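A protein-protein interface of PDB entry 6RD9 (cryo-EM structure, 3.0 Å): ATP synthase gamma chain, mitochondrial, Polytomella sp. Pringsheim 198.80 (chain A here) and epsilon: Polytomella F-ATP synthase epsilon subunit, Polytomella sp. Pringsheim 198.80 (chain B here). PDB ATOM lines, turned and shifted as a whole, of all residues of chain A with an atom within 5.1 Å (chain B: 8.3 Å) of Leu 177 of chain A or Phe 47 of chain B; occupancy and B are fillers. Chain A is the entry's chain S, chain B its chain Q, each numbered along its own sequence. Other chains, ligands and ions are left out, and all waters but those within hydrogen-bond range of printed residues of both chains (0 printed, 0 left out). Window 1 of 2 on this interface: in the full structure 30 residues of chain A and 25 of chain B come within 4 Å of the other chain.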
ATOM      1  N   ILE A 162     -15.468  17.733  12.600  1.00  0.00           N
ATOM      2  CA  ILE A 162     -14.363  16.796  12.454  1.00  0.00           C
ATOM      3  C   ILE A 162     -14.901  15.531  11.806  1.00  0.00           C
ATOM      4  O   ILE A 162     -15.896  14.963  12.262  1.00  0.00           O
ATOM      5  CB  ILE A 162     -13.702  16.479  13.806  1.00  0.00           C
ATOM      6  CG1 ILE A 162     -13.056  17.711  14.432  1.00  0.00           C
ATOM      7  CG2 ILE A 162     -12.623  15.449  13.632  1.00  0.00           C
ATOM      8  CD1 ILE A 162     -13.868  18.361  15.498  1.00  0.00           C
ATOM      9  N   ALA A 163     -14.264  15.099  10.728  1.00  0.00           N
ATOM     10  CA  ALA A 163     -14.628  13.861  10.077  1.00  0.00           C
ATOM     11  C   ALA A 163     -13.352  13.138   9.699  1.00  0.00           C
ATOM     12  O   ALA A 163     -12.254  13.581  10.040  1.00  0.00           O
ATOM     13  CB  ALA A 163     -15.524  14.122   8.866  1.00  0.00           C
ATOM     14  N   ASP A 164     -13.518  12.006   9.008  1.00  0.00           N
ATOM     15  CA  ASP A 164     -12.438  11.132   8.540  1.00  0.00           C
ATOM     16  C   ASP A 164     -11.577  10.621   9.690  1.00  0.00           C
ATOM     17  O   ASP A 164     -10.390  10.348   9.515  1.00  0.00           O
ATOM     18  CB  ASP A 164     -11.573  11.822   7.483  1.00  0.00           C
ATOM     19  CG  ASP A 164     -11.997  11.485   6.070  1.00  0.00           C
ATOM     20  OD1 ASP A 164     -11.410  12.057   5.125  1.00  0.00           O
ATOM     21  OD2 ASP A 164     -12.909  10.647   5.903  1.00  0.00           O
ATOM     22  N   THR A 165     -12.182  10.472  10.866  1.00  0.00           N
ATOM     23  CA  THR A 165     -11.436  10.154  12.076  1.00  0.00           C
ATOM     24  C   THR A 165     -11.039   8.689  12.128  1.00  0.00           C
ATOM     25  O   THR A 165      -9.866   8.363  12.334  1.00  0.00           O
ATOM     26  CB  THR A 165     -12.269  10.506  13.302  1.00  0.00           C
ATOM     27  OG1 THR A 165     -12.475  11.918  13.361  1.00  0.00           O
ATOM     28  CG2 THR A 165     -11.585  10.072  14.538  1.00  0.00           C
ATOM     29  N   PHE A 172      -4.152   9.090  20.217  1.00  0.00           N
ATOM     30  CA  PHE A 172      -4.219  10.184  21.173  1.00  0.00           C
ATOM     31  C   PHE A 172      -3.663  11.474  20.605  1.00  0.00           C
ATOM     32  O   PHE A 172      -4.118  12.552  20.995  1.00  0.00           O
ATOM     33  CB  PHE A 172      -3.474   9.831  22.450  1.00  0.00           C
ATOM     34  CG  PHE A 172      -3.793  10.736  23.586  1.00  0.00           C
ATOM     35  CD1 PHE A 172      -2.998  11.822  23.877  1.00  0.00           C
ATOM     36  CD2 PHE A 172      -4.896  10.502  24.359  1.00  0.00           C
ATOM     37  CE1 PHE A 172      -3.308  12.649  24.900  1.00  0.00           C
ATOM     38  CE2 PHE A 172      -5.197  11.320  25.383  1.00  0.00           C
ATOM     39  CZ  PHE A 172      -4.405  12.396  25.656  1.00  0.00           C
ATOM     40  N   GLY A 173      -2.674  11.396  19.716  1.00  0.00           N
ATOM     41  CA  GLY A 173      -2.192  12.604  19.071  1.00  0.00           C
ATOM     42  C   GLY A 173      -3.237  13.217  18.167  1.00  0.00           C
ATOM     43  O   GLY A 173      -3.330  14.439  18.042  1.00  0.00           O
ATOM     44  N   GLN A 174      -4.050  12.371  17.538  1.00  0.00           N
ATOM     45  CA  GLN A 174      -5.185  12.847  16.763  1.00  0.00           C
ATOM     46  C   GLN A 174      -6.242  13.451  17.669  1.00  0.00           C
ATOM     47  O   GLN A 174      -6.803  14.506  17.368  1.00  0.00           O
ATOM     48  CB  GLN A 174      -5.749  11.688  15.954  1.00  0.00           C
ATOM     49  CG  GLN A 174      -7.098  11.883  15.353  1.00  0.00           C
ATOM     50  CD  GLN A 174      -7.562  10.624  14.691  1.00  0.00           C
ATOM     51  OE1 GLN A 174      -7.114   9.535  15.033  1.00  0.00           O
ATOM     52  NE2 GLN A 174      -8.423  10.760  13.714  1.00  0.00           N
ATOM     53  N   ALA A 175      -6.508  12.806  18.803  1.00  0.00           N
ATOM     54  CA  ALA A 175      -7.463  13.355  19.753  1.00  0.00           C
ATOM     55  C   ALA A 175      -6.899  14.554  20.493  1.00  0.00           C
ATOM     56  O   ALA A 175      -7.655  15.319  21.093  1.00  0.00           O
ATOM     57  CB  ALA A 175      -7.883  12.283  20.738  1.00  0.00           C
ATOM     58  N   SER A 176      -5.576  14.720  20.491  1.00  0.00           N
ATOM     59  CA  SER A 176      -4.993  15.943  21.022  1.00  0.00           C
ATOM     60  C   SER A 176      -5.254  17.117  20.095  1.00  0.00           C
ATOM     61  O   SER A 176      -5.655  18.188  20.555  1.00  0.00           O
ATOM     62  CB  SER A 176      -3.497  15.767  21.223  1.00  0.00           C
ATOM     63  OG  SER A 176      -3.224  14.766  22.178  1.00  0.00           O
ATOM     64  N   LEU A 177      -5.060  16.922  18.787  1.00  0.00           N
ATOM     65  CA  LEU A 177      -5.251  17.996  17.815  1.00  0.00           C
ATOM     66  C   LEU A 177      -6.701  18.426  17.738  1.00  0.00           C
ATOM     67  O   LEU A 177      -6.992  19.602  17.512  1.00  0.00           O
ATOM     68  CB  LEU A 177      -4.796  17.545  16.436  1.00  0.00           C
ATOM     69  CG  LEU A 177      -3.321  17.332  16.189  1.00  0.00           C
ATOM     70  CD1 LEU A 177      -3.131  17.001  14.740  1.00  0.00           C
ATOM     71  CD2 LEU A 177      -2.569  18.586  16.552  1.00  0.00           C
ATOM     72  N   ILE A 178      -7.625  17.483  17.909  1.00  0.00           N
ATOM     73  CA  ILE A 178      -9.041  17.819  17.971  1.00  0.00           C
ATOM     74  C   ILE A 178      -9.324  18.623  19.225  1.00  0.00           C
ATOM     75  O   ILE A 178     -10.154  19.537  19.224  1.00  0.00           O
ATOM     76  CB  ILE A 178      -9.886  16.534  17.897  1.00  0.00           C
ATOM     77  CG1 ILE A 178      -9.617  15.823  16.583  1.00  0.00           C
ATOM     78  CG2 ILE A 178     -11.349  16.821  17.953  1.00  0.00           C
ATOM     79  CD1 ILE A 178     -10.165  14.444  16.522  1.00  0.00           C
ATOM     80  N   VAL A 179      -8.607  18.321  20.305  1.00  0.00           N
ATOM     81  CA  VAL A 179      -8.792  19.069  21.539  1.00  0.00           C
ATOM     82  C   VAL A 179      -8.170  20.453  21.449  1.00  0.00           C
ATOM     83  O   VAL A 179      -8.738  21.410  21.969  1.00  0.00           O
ATOM     84  CB  VAL A 179      -8.221  18.292  22.719  1.00  0.00           C
ATOM     85  N   GLU A 180      -7.034  20.597  20.756  1.00  0.00           N
ATOM     86  CA  GLU A 180      -6.411  21.917  20.645  1.00  0.00           C
ATOM     87  C   GLU A 180      -7.223  22.850  19.759  1.00  0.00           C
ATOM     88  O   GLU A 180      -7.202  24.069  19.949  1.00  0.00           O
ATOM     89  CB  GLU A 180      -4.982  21.818  20.123  1.00  0.00           C
ATOM     90  CG  GLU A 180      -4.080  20.962  20.955  1.00  0.00           C
ATOM     91  CD  GLU A 180      -2.860  20.509  20.202  1.00  0.00           C
ATOM     92  OE1 GLU A 180      -2.378  21.272  19.340  1.00  0.00           O
ATOM     93  OE2 GLU A 180      -2.385  19.386  20.466  1.00  0.00           O
ATOM     94  N   GLU A 181      -7.950  22.297  18.788  1.00  0.00           N
ATOM     95  CA  GLU A 181      -8.875  23.116  18.015  1.00  0.00           C
ATOM     96  C   GLU A 181     -10.101  23.493  18.835  1.00  0.00           C
ATOM     97  O   GLU A 181     -10.812  24.436  18.482  1.00  0.00           O
ATOM     98  CB  GLU A 181      -9.293  22.385  16.746  1.00  0.00           C
ATOM     99  CG  GLU A 181      -8.152  22.093  15.775  1.00  0.00           C
ATOM    100  CD  GLU A 181      -7.568  23.328  15.118  1.00  0.00           C
ATOM    101  OE1 GLU A 181      -8.314  24.304  14.888  1.00  0.00           O
ATOM    102  OE2 GLU A 181      -6.358  23.317  14.815  1.00  0.00           O
ATOM    103  N   SER B  15       0.233  24.535  23.573  1.00  0.00           N
ATOM    104  CA  SER B  15      -0.595  23.922  24.592  1.00  0.00           C
ATOM    105  C   SER B  15       0.153  22.765  25.241  1.00  0.00           C
ATOM    106  O   SER B  15       1.180  22.301  24.743  1.00  0.00           O
ATOM    107  CB  SER B  15      -1.905  23.432  23.987  1.00  0.00           C
ATOM    108  OG  SER B  15      -1.693  22.253  23.234  1.00  0.00           O
ATOM    109  N   LEU B  17      -1.070  19.759  25.549  1.00  0.00           N
ATOM    110  CA  LEU B  17      -1.357  18.554  24.780  1.00  0.00           C
ATOM    111  C   LEU B  17      -0.387  18.383  23.632  1.00  0.00           C
ATOM    112  O   LEU B  17       0.008  17.259  23.310  1.00  0.00           O
ATOM    113  CB  LEU B  17      -2.770  18.607  24.230  1.00  0.00           C
ATOM    114  CG  LEU B  17      -3.868  18.389  25.236  1.00  0.00           C
ATOM    115  CD1 LEU B  17      -5.112  18.922  24.610  1.00  0.00           C
ATOM    116  CD2 LEU B  17      -3.979  16.918  25.519  1.00  0.00           C
ATOM    117  N   ARG B  18       0.001  19.485  22.995  1.00  0.00           N
ATOM    118  CA  ARG B  18       0.985  19.378  21.935  1.00  0.00           C
ATOM    119  C   ARG B  18       2.354  19.068  22.500  1.00  0.00           C
ATOM    120  O   ARG B  18       3.071  18.232  21.950  1.00  0.00           O
ATOM    121  CB  ARG B  18       1.039  20.654  21.112  1.00  0.00           C
ATOM    122  CG  ARG B  18       1.799  20.449  19.829  1.00  0.00           C
ATOM    123  CD  ARG B  18       1.760  21.668  18.972  1.00  0.00           C
ATOM    124  NE  ARG B  18       0.447  21.859  18.387  1.00  0.00           N
ATOM    125  CZ  ARG B  18       0.130  21.469  17.163  1.00  0.00           C
ATOM    126  NH1 ARG B  18       1.032  20.863  16.405  1.00  0.00           N
ATOM    127  NH2 ARG B  18      -1.089  21.683  16.701  1.00  0.00           N
ATOM    128  N   ASN B  21       2.620  15.459  23.661  1.00  0.00           N
ATOM    129  CA  ASN B  21       2.643  14.529  22.540  1.00  0.00           C
ATOM    130  C   ASN B  21       3.931  14.611  21.739  1.00  0.00           C
ATOM    131  O   ASN B  21       4.328  13.609  21.139  1.00  0.00           O
ATOM    132  CB  ASN B  21       1.449  14.766  21.624  1.00  0.00           C
ATOM    133  CG  ASN B  21       0.269  13.926  22.004  1.00  0.00           C
ATOM    134  OD1 ASN B  21       0.222  12.745  21.692  1.00  0.00           O
ATOM    135  ND2 ASN B  21      -0.696  14.524  22.675  1.00  0.00           N
ATOM    136  N   GLN B  43       1.048   6.497  16.593  1.00  0.00           N
ATOM    137  CA  GLN B  43       1.594   7.820  16.354  1.00  0.00           C
ATOM    138  C   GLN B  43       0.885   8.562  15.238  1.00  0.00           C
ATOM    139  O   GLN B  43       0.919   9.797  15.219  1.00  0.00           O
ATOM    140  CB  GLN B  43       3.083   7.704  16.012  1.00  0.00           C
ATOM    141  CG  GLN B  43       3.901   8.949  16.253  1.00  0.00           C
ATOM    142  CD  GLN B  43       5.378   8.647  16.314  1.00  0.00           C
ATOM    143  OE1 GLN B  43       5.776   7.496  16.477  1.00  0.00           O
ATOM    144  NE2 GLN B  43       6.201   9.678  16.191  1.00  0.00           N
ATOM    145  N   ALA B  44       0.244   7.845  14.317  1.00  0.00           N
ATOM    146  CA  ALA B  44      -0.280   8.453  13.105  1.00  0.00           C
ATOM    147  C   ALA B  44      -1.505   9.307  13.398  1.00  0.00           C
ATOM    148  O   ALA B  44      -2.281   9.044  14.315  1.00  0.00           O
ATOM    149  CB  ALA B  44      -0.637   7.380  12.081  1.00  0.00           C
ATOM    150  N   ILE B  45      -1.675  10.347  12.593  1.00  0.00           N
ATOM    151  CA  ILE B  45      -2.802  11.259  12.718  1.00  0.00           C
ATOM    152  C   ILE B  45      -3.454  11.375  11.352  1.00  0.00           C
ATOM    153  O   ILE B  45      -2.851  11.911  10.416  1.00  0.00           O
ATOM    154  CB  ILE B  45      -2.375  12.639  13.233  1.00  0.00           C
ATOM    155  CG1 ILE B  45      -1.904  12.538  14.678  1.00  0.00           C
ATOM    156  CG2 ILE B  45      -3.522  13.614  13.134  1.00  0.00           C
ATOM    157  CD1 ILE B  45      -1.257  13.789  15.185  1.00  0.00           C
ATOM    158  N   HIS B  46      -4.679  10.870  11.236  1.00  0.00           N
ATOM    159  CA  HIS B  46      -5.430  10.915   9.985  1.00  0.00           C
ATOM    160  C   HIS B  46      -6.843  11.352  10.338  1.00  0.00           C
ATOM    161  O   HIS B  46      -7.636  10.536  10.809  1.00  0.00           O
ATOM    162  CB  HIS B  46      -5.455   9.567   9.276  1.00  0.00           C
ATOM    163  CG  HIS B  46      -4.112   9.047   8.879  1.00  0.00           C
ATOM    164  ND1 HIS B  46      -3.498   8.004   9.532  1.00  0.00           N
ATOM    165  CD2 HIS B  46      -3.277   9.410   7.879  1.00  0.00           C
ATOM    166  CE1 HIS B  46      -2.337   7.749   8.957  1.00  0.00           C
ATOM    167  NE2 HIS B  46      -2.179   8.590   7.952  1.00  0.00           N
ATOM    168  N   PHE B  47      -7.152  12.620  10.110  1.00  0.00           N
ATOM    169  CA  PHE B  47      -8.520  13.108  10.195  1.00  0.00           C
ATOM    170  C   PHE B  47      -8.619  14.348   9.322  1.00  0.00           C
ATOM    171  O   PHE B  47      -7.747  14.604   8.488  1.00  0.00           O
ATOM    172  CB  PHE B  47      -8.957  13.344  11.650  1.00  0.00           C
ATOM    173  CG  PHE B  47      -8.352  14.550  12.311  1.00  0.00           C
ATOM    174  CD1 PHE B  47      -7.025  14.563  12.696  1.00  0.00           C
ATOM    175  CD2 PHE B  47      -9.140  15.644  12.616  1.00  0.00           C
ATOM    176  CE1 PHE B  47      -6.491  15.658  13.317  1.00  0.00           C
ATOM    177  CE2 PHE B  47      -8.607  16.741  13.237  1.00  0.00           C
ATOM    178  CZ  PHE B  47      -7.285  16.746  13.590  1.00  0.00           C
ATOM    179  N   ARG B  48      -9.711  15.085   9.468  1.00  0.00           N
ATOM    180  CA  ARG B  48      -9.880  16.360   8.798  1.00  0.00           C
ATOM    181  C   ARG B  48     -10.849  17.185   9.625  1.00  0.00           C
ATOM    182  O   ARG B  48     -11.595  16.644  10.441  1.00  0.00           O
ATOM    183  CB  ARG B  48     -10.407  16.192   7.373  1.00  0.00           C
ATOM    184  CG  ARG B  48     -11.791  15.604   7.339  1.00  0.00           C
ATOM    185  CD  ARG B  48     -12.429  15.649   5.987  1.00  0.00           C
ATOM    186  NE  ARG B  48     -13.830  15.293   6.140  1.00  0.00           N
ATOM    187  CZ  ARG B  48     -14.745  15.368   5.186  1.00  0.00           C
ATOM    188  NH1 ARG B  48     -15.994  15.023   5.452  1.00  0.00           N
ATOM    189  NH2 ARG B  48     -14.412  15.790   3.977  1.00  0.00           N
ATOM    190  N   GLN B  49     -10.821  18.498   9.430  1.00  0.00           N
ATOM    191  CA  GLN B  49     -11.730  19.377  10.146  1.00  0.00           C
ATOM    192  C   GLN B  49     -12.310  20.393   9.180  1.00  0.00           C
ATOM    193  O   GLN B  49     -11.815  20.576   8.069  1.00  0.00           O
ATOM    194  CB  GLN B  49     -11.037  20.090  11.313  1.00  0.00           C
ATOM    195  CG  GLN B  49     -10.143  21.217  10.893  1.00  0.00           C
ATOM    196  CD  GLN B  49      -9.258  21.702  12.010  1.00  0.00           C
ATOM    197  OE1 GLN B  49      -8.111  21.276  12.137  1.00  0.00           O
ATOM    198  NE2 GLN B  49      -9.785  22.598  12.832  1.00  0.00           N
ATOM    199  N   ALA B  50     -13.380  21.055   9.617  1.00  0.00           N
ATOM    200  CA  ALA B  50     -14.043  22.037   8.807  1.00  0.00           C
ATOM    201  C   ALA B  50     -14.790  22.993   9.722  1.00  0.00           C
ATOM    202  O   ALA B  50     -15.574  22.534  10.566  1.00  0.00           O
ATOM    203  CB  ALA B  50     -15.015  21.410   7.813  1.00  0.00           C
ATOM    204  N   LYS B  61      -9.119  21.684   6.801  1.00  0.00           N
ATOM    205  CA  LYS B  61      -7.769  21.323   7.207  1.00  0.00           C
ATOM    206  C   LYS B  61      -7.669  19.809   7.334  1.00  0.00           C
ATOM    207  O   LYS B  61      -8.118  19.237   8.330  1.00  0.00           O
ATOM    208  CB  LYS B  61      -7.440  22.010   8.527  1.00  0.00           C
ATOM    209  CG  LYS B  61      -6.062  21.726   9.055  1.00  0.00           C
ATOM    210  CD  LYS B  61      -4.978  22.456   8.312  1.00  0.00           C
ATOM    211  CE  LYS B  61      -3.644  22.015   8.850  1.00  0.00           C
ATOM    212  NZ  LYS B  61      -3.555  22.279  10.313  1.00  0.00           N
ATOM    213  N   VAL B  62      -7.102  19.152   6.329  1.00  0.00           N
ATOM    214  CA  VAL B  62      -6.978  17.701   6.326  1.00  0.00           C
ATOM    215  C   VAL B  62      -5.603  17.322   6.851  1.00  0.00           C
ATOM    216  O   VAL B  62      -4.663  18.126   6.820  1.00  0.00           O
ATOM    217  CB  VAL B  62      -7.239  17.105   4.928  1.00  0.00           C
ATOM    218  CG1 VAL B  62      -8.488  17.724   4.315  1.00  0.00           C
ATOM    219  CG2 VAL B  62      -6.040  17.263   4.002  1.00  0.00           C
ATOM    220  N   TYR B  63      -5.500  16.113   7.393  1.00  0.00           N
ATOM    221  CA  TYR B  63      -4.264  15.596   7.956  1.00  0.00           C
ATOM    222  C   TYR B  63      -4.032  14.196   7.414  1.00  0.00           C
ATOM    223  O   TYR B  63      -4.929  13.352   7.482  1.00  0.00           O
ATOM    224  CB  TYR B  63      -4.335  15.557   9.483  1.00  0.00           C
ATOM    225  CG  TYR B  63      -4.506  16.903  10.145  1.00  0.00           C
ATOM    226  CD1 TYR B  63      -5.768  17.435  10.366  1.00  0.00           C
ATOM    227  CD2 TYR B  63      -3.410  17.630  10.575  1.00  0.00           C
ATOM    228  CE1 TYR B  63      -5.933  18.659  10.973  1.00  0.00           C
ATOM    229  CE2 TYR B  63      -3.564  18.854  11.186  1.00  0.00           C
ATOM    230  CZ  TYR B  63      -4.830  19.364  11.385  1.00  0.00           C
ATOM    231  OH  TYR B  63      -4.996  20.588  11.996  1.00  0.00           O
ATOM    232  N   GLU B  64      -2.848  13.948   6.867  1.00  0.00           N
ATOM    233  CA  GLU B  64      -2.413  12.597   6.516  1.00  0.00           C
ATOM    234  C   GLU B  64      -1.036  12.338   7.115  1.00  0.00           C
ATOM    235  O   GLU B  64      -0.112  11.820   6.484  1.00  0.00           O
ATOM    236  CB  GLU B  64      -2.478  12.347   5.001  1.00  0.00           C
ATOM    237  CG  GLU B  64      -1.681  13.285   4.098  1.00  0.00           C
ATOM    238  CD  GLU B  64      -2.500  14.454   3.594  1.00  0.00           C
ATOM    239  OE1 GLU B  64      -3.584  14.726   4.151  1.00  0.00           O
ATOM    240  OE2 GLU B  64      -2.054  15.098   2.624  1.00  0.00           O
ATOM    241  N   LEU B  65      -0.930  12.667   8.397  1.00  0.00           N
ATOM    242  CA  LEU B  65       0.324  12.646   9.136  1.00  0.00           C
ATOM    243  C   LEU B  65       0.645  11.226   9.577  1.00  0.00           C
ATOM    244  O   LEU B  65      -0.239  10.500  10.037  1.00  0.00           O
ATOM    245  CB  LEU B  65       0.205  13.558  10.350  1.00  0.00           C
ATOM    246  CG  LEU B  65       0.425  15.068  10.299  1.00  0.00           C
ATOM    247  CD1 LEU B  65      -0.525  15.808   9.378  1.00  0.00           C
ATOM    248  CD2 LEU B  65       0.233  15.577  11.690  1.00  0.00           C
ATOM    249  N   GLY B  68       3.902  11.801  13.356  1.00  0.00           N
ATOM    250  CA  GLY B  68       3.399  12.256  14.628  1.00  0.00           C
ATOM    251  C   GLY B  68       2.854  13.660  14.546  1.00  0.00           C
ATOM    252  O   GLY B  68       2.660  14.216  13.469  1.00  0.00           O
ATOM    253  N   ILE B  69       2.598  14.218  15.722  1.00  0.00           N
ATOM    254  CA  ILE B  69       2.052  15.571  15.851  1.00  0.00           C
ATOM    255  C   ILE B  69       3.127  16.568  15.421  1.00  0.00           C
ATOM    256  O   ILE B  69       4.329  16.280  15.594  1.00  0.00           O
ATOM    257  CB  ILE B  69       1.572  15.792  17.305  1.00  0.00           C
ATOM    258  CG1 ILE B  69       0.649  16.992  17.481  1.00  0.00           C
ATOM    259  CG2 ILE B  69       2.708  15.893  18.306  1.00  0.00           C
ATOM    260  CD1 ILE B  69      -0.005  17.019  18.834  1.00  0.00           C
ATOM    261  N   PRO B  70       2.781  17.674  14.751  1.00  0.00           N
ATOM    262  CA  PRO B  70       3.826  18.527  14.169  1.00  0.00           C
ATOM    263  C   PRO B  70       4.646  19.255  15.225  1.00  0.00           C
ATOM    264  O   PRO B  70       4.102  19.907  16.120  1.00  0.00           O
ATOM    265  CB  PRO B  70       3.038  19.508  13.296  1.00  0.00           C
ATOM    266  CG  PRO B  70       1.814  18.785  12.959  1.00  0.00           C
ATOM    267  CD  PRO B  70       1.466  17.998  14.173  1.00  0.00           C
ATOM    268  N   ASN B  74       2.085  25.802  14.710  1.00  0.00           N
ATOM    269  CA  ASN B  74       0.777  25.541  14.121  1.00  0.00           C
ATOM    270  C   ASN B  74       0.185  26.804  13.502  1.00  0.00           C
ATOM    271  O   ASN B  74      -0.086  26.855  12.300  1.00  0.00           O
ATOM    272  CB  ASN B  74      -0.170  24.972  15.178  1.00  0.00           C
ATOM    273  CG  ASN B  74      -0.395  25.927  16.333  1.00  0.00           C
ATOM    274  OD1 ASN B  74       0.490  26.702  16.698  1.00  0.00           O
ATOM    275  ND2 ASN B  74      -1.579  25.868  16.926  1.00  0.00           N
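Of the printed residues of chain B, Ile 162 of chain A touches Phe 47 and Arg 48. Of the printed residues of chain B, Thr 165 of chain A touches His 46. Of the printed residues of chain B, Leu 177 of chain A touches Arg 18 (3.4 Å), Ile 45 (3.7 Å), Phe 47 (3.9 Å) and Ile 69 (3.7 Å). Printed residues of chain B within 4 Å of Ile 178 of chain A: Phe 47. Of the printed residues of chain A, Ile 45 of chain B touches Gly 173 (3.6 Å), Gln 174 (3.6 Å) and Leu 177 (3.7 Å). Printed residues of chain A within 4 Å of Phe 47 of chain B: Ile 162 (3.6 Å), Ala 163 (3.7 Å), Asp 164 (3.4 Å), Gln 174 (3.3 Å), Leu 177 (3.9 Å) and Ile 178 (3.6 Å). The nearest residue of chain B that does not touch Leu 177 of chain A is Tyr 63 of chain B (4.03 Å). The nearest residue of chain A that does not touch Phe 47 of chain B is Thr 165 of chain A (4.1 Å). The nearest printed residue of chain A that does not touch Ser 15 of chain B is Ser 176 of chain A (6.3 Å).
Among the printed residues, pairs that only touch across the chains: Gln 174 of chain A with Phe 47 of chain B (3.3 Å), Asp 164 of chain A with Phe 47 of chain B (3.4 Å), Ile 162 of chain A with Arg 48 of chain B (3.4 Å), Leu 177 of chain A with Arg 18 of chain B (3.4 Å), Glu 180 of chain A with Ser 15 of chain B (3.5 Å), Gly 173 of chain A with Asn 21 of chain B (3.6 Å), Gln 174 of chain A with Ile 45 of chain B (3.6 Å), Gly 173 of chain A with Ile 45 of chain B (3.6 Å), Ile 178 of chain A with Phe 47 of chain B (3.6 Å), Ile 162 of chain A with Phe 47 of chain B (3.6 Å), Ala 163 of chain A with Phe 47 of chain B (3.7 Å), Val 179 of chain A with Leu 17 of chain B (3.7 Å), Leu 177 of chain A with Ile 69 of chain B (3.7 Å), Glu 180 of chain A with Ile 69 of chain B (3.7 Å), Leu 177 of chain A with Ile 45 of chain B (3.7 Å), Phe 172 of chain A with Asn 21 of chain B (3.7 Å), Asp 164 of chain A with Arg 48 of chain B (3.8 Å), Glu 180 of chain A with Leu 17 of chain B (3.9 Å) and Leu 177 of chain A with Phe 47 of chain B (3.9 Å).
O of Phe 47 of chain B sits at hydrogen-bond distance from N of Tyr 63 of chain B (2.9 Å). The side-chain hydroxyl (OG) of Ser 15 of chain B sits close to the backbone NH (N) of Leu 17 of chain B (3.5 Å). The backbone carbonyl oxygen (O) of Thr 165 of chain A sits at hydrogen-bond distance from the side-chain amide nitrogen (NE2) of Gln 174 of chain A. O of Leu 17 of chain B sits at hydrogen-bond distance from ND2 of Asn 21 of chain B (2.9 Å). The side-chain amide oxygen (OE1) of Gln 49 of chain B lies within hydrogen-bond range of the side-chain hydroxyl (OH) of Tyr 63 of chain B. O of Lys 61 of chain B lies within hydrogen-bond range of N of Gln 49 of chain B (3.0 Å).
O of Thr 165 of chain A sits close to O of His 46 of chain B, 3.5 Å away. The guanidinium group (NH2) of Arg 18 of chain B lies within salt-bridge range of the side-chain carboxylate (OE1) of Glu 180 of chain A (3.0 Å). OG of Ser 176 of chain A is in hydrogen-bond range of ND2 of Asn 21 of chain B, 2.6 Å away. O of His 46 of chain B sits close to O of Asp 164 of chain A. NE2 of Gln 49 of chain B is in hydrogen-bond range of OE1 of Glu 181 of chain A, at 3.0 Å. O of His 46 of chain B is in hydrogen-bond range of NE2 of Gln 174 of chain A (3.0 Å). The backbone NH of Arg 48 of chain B sits at hydrogen-bond distance from the backbone carbonyl oxygen of Ala 163 of chain A (3.0 Å).
Of the 14 printed residues of chain A, 13 touch a printed residue of chain B. Hydrophobic or aromatic side chains of chain B within 4 Å of the printed part of chain A: Leu 17, Ile 45, Phe 47 and Ile 69.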
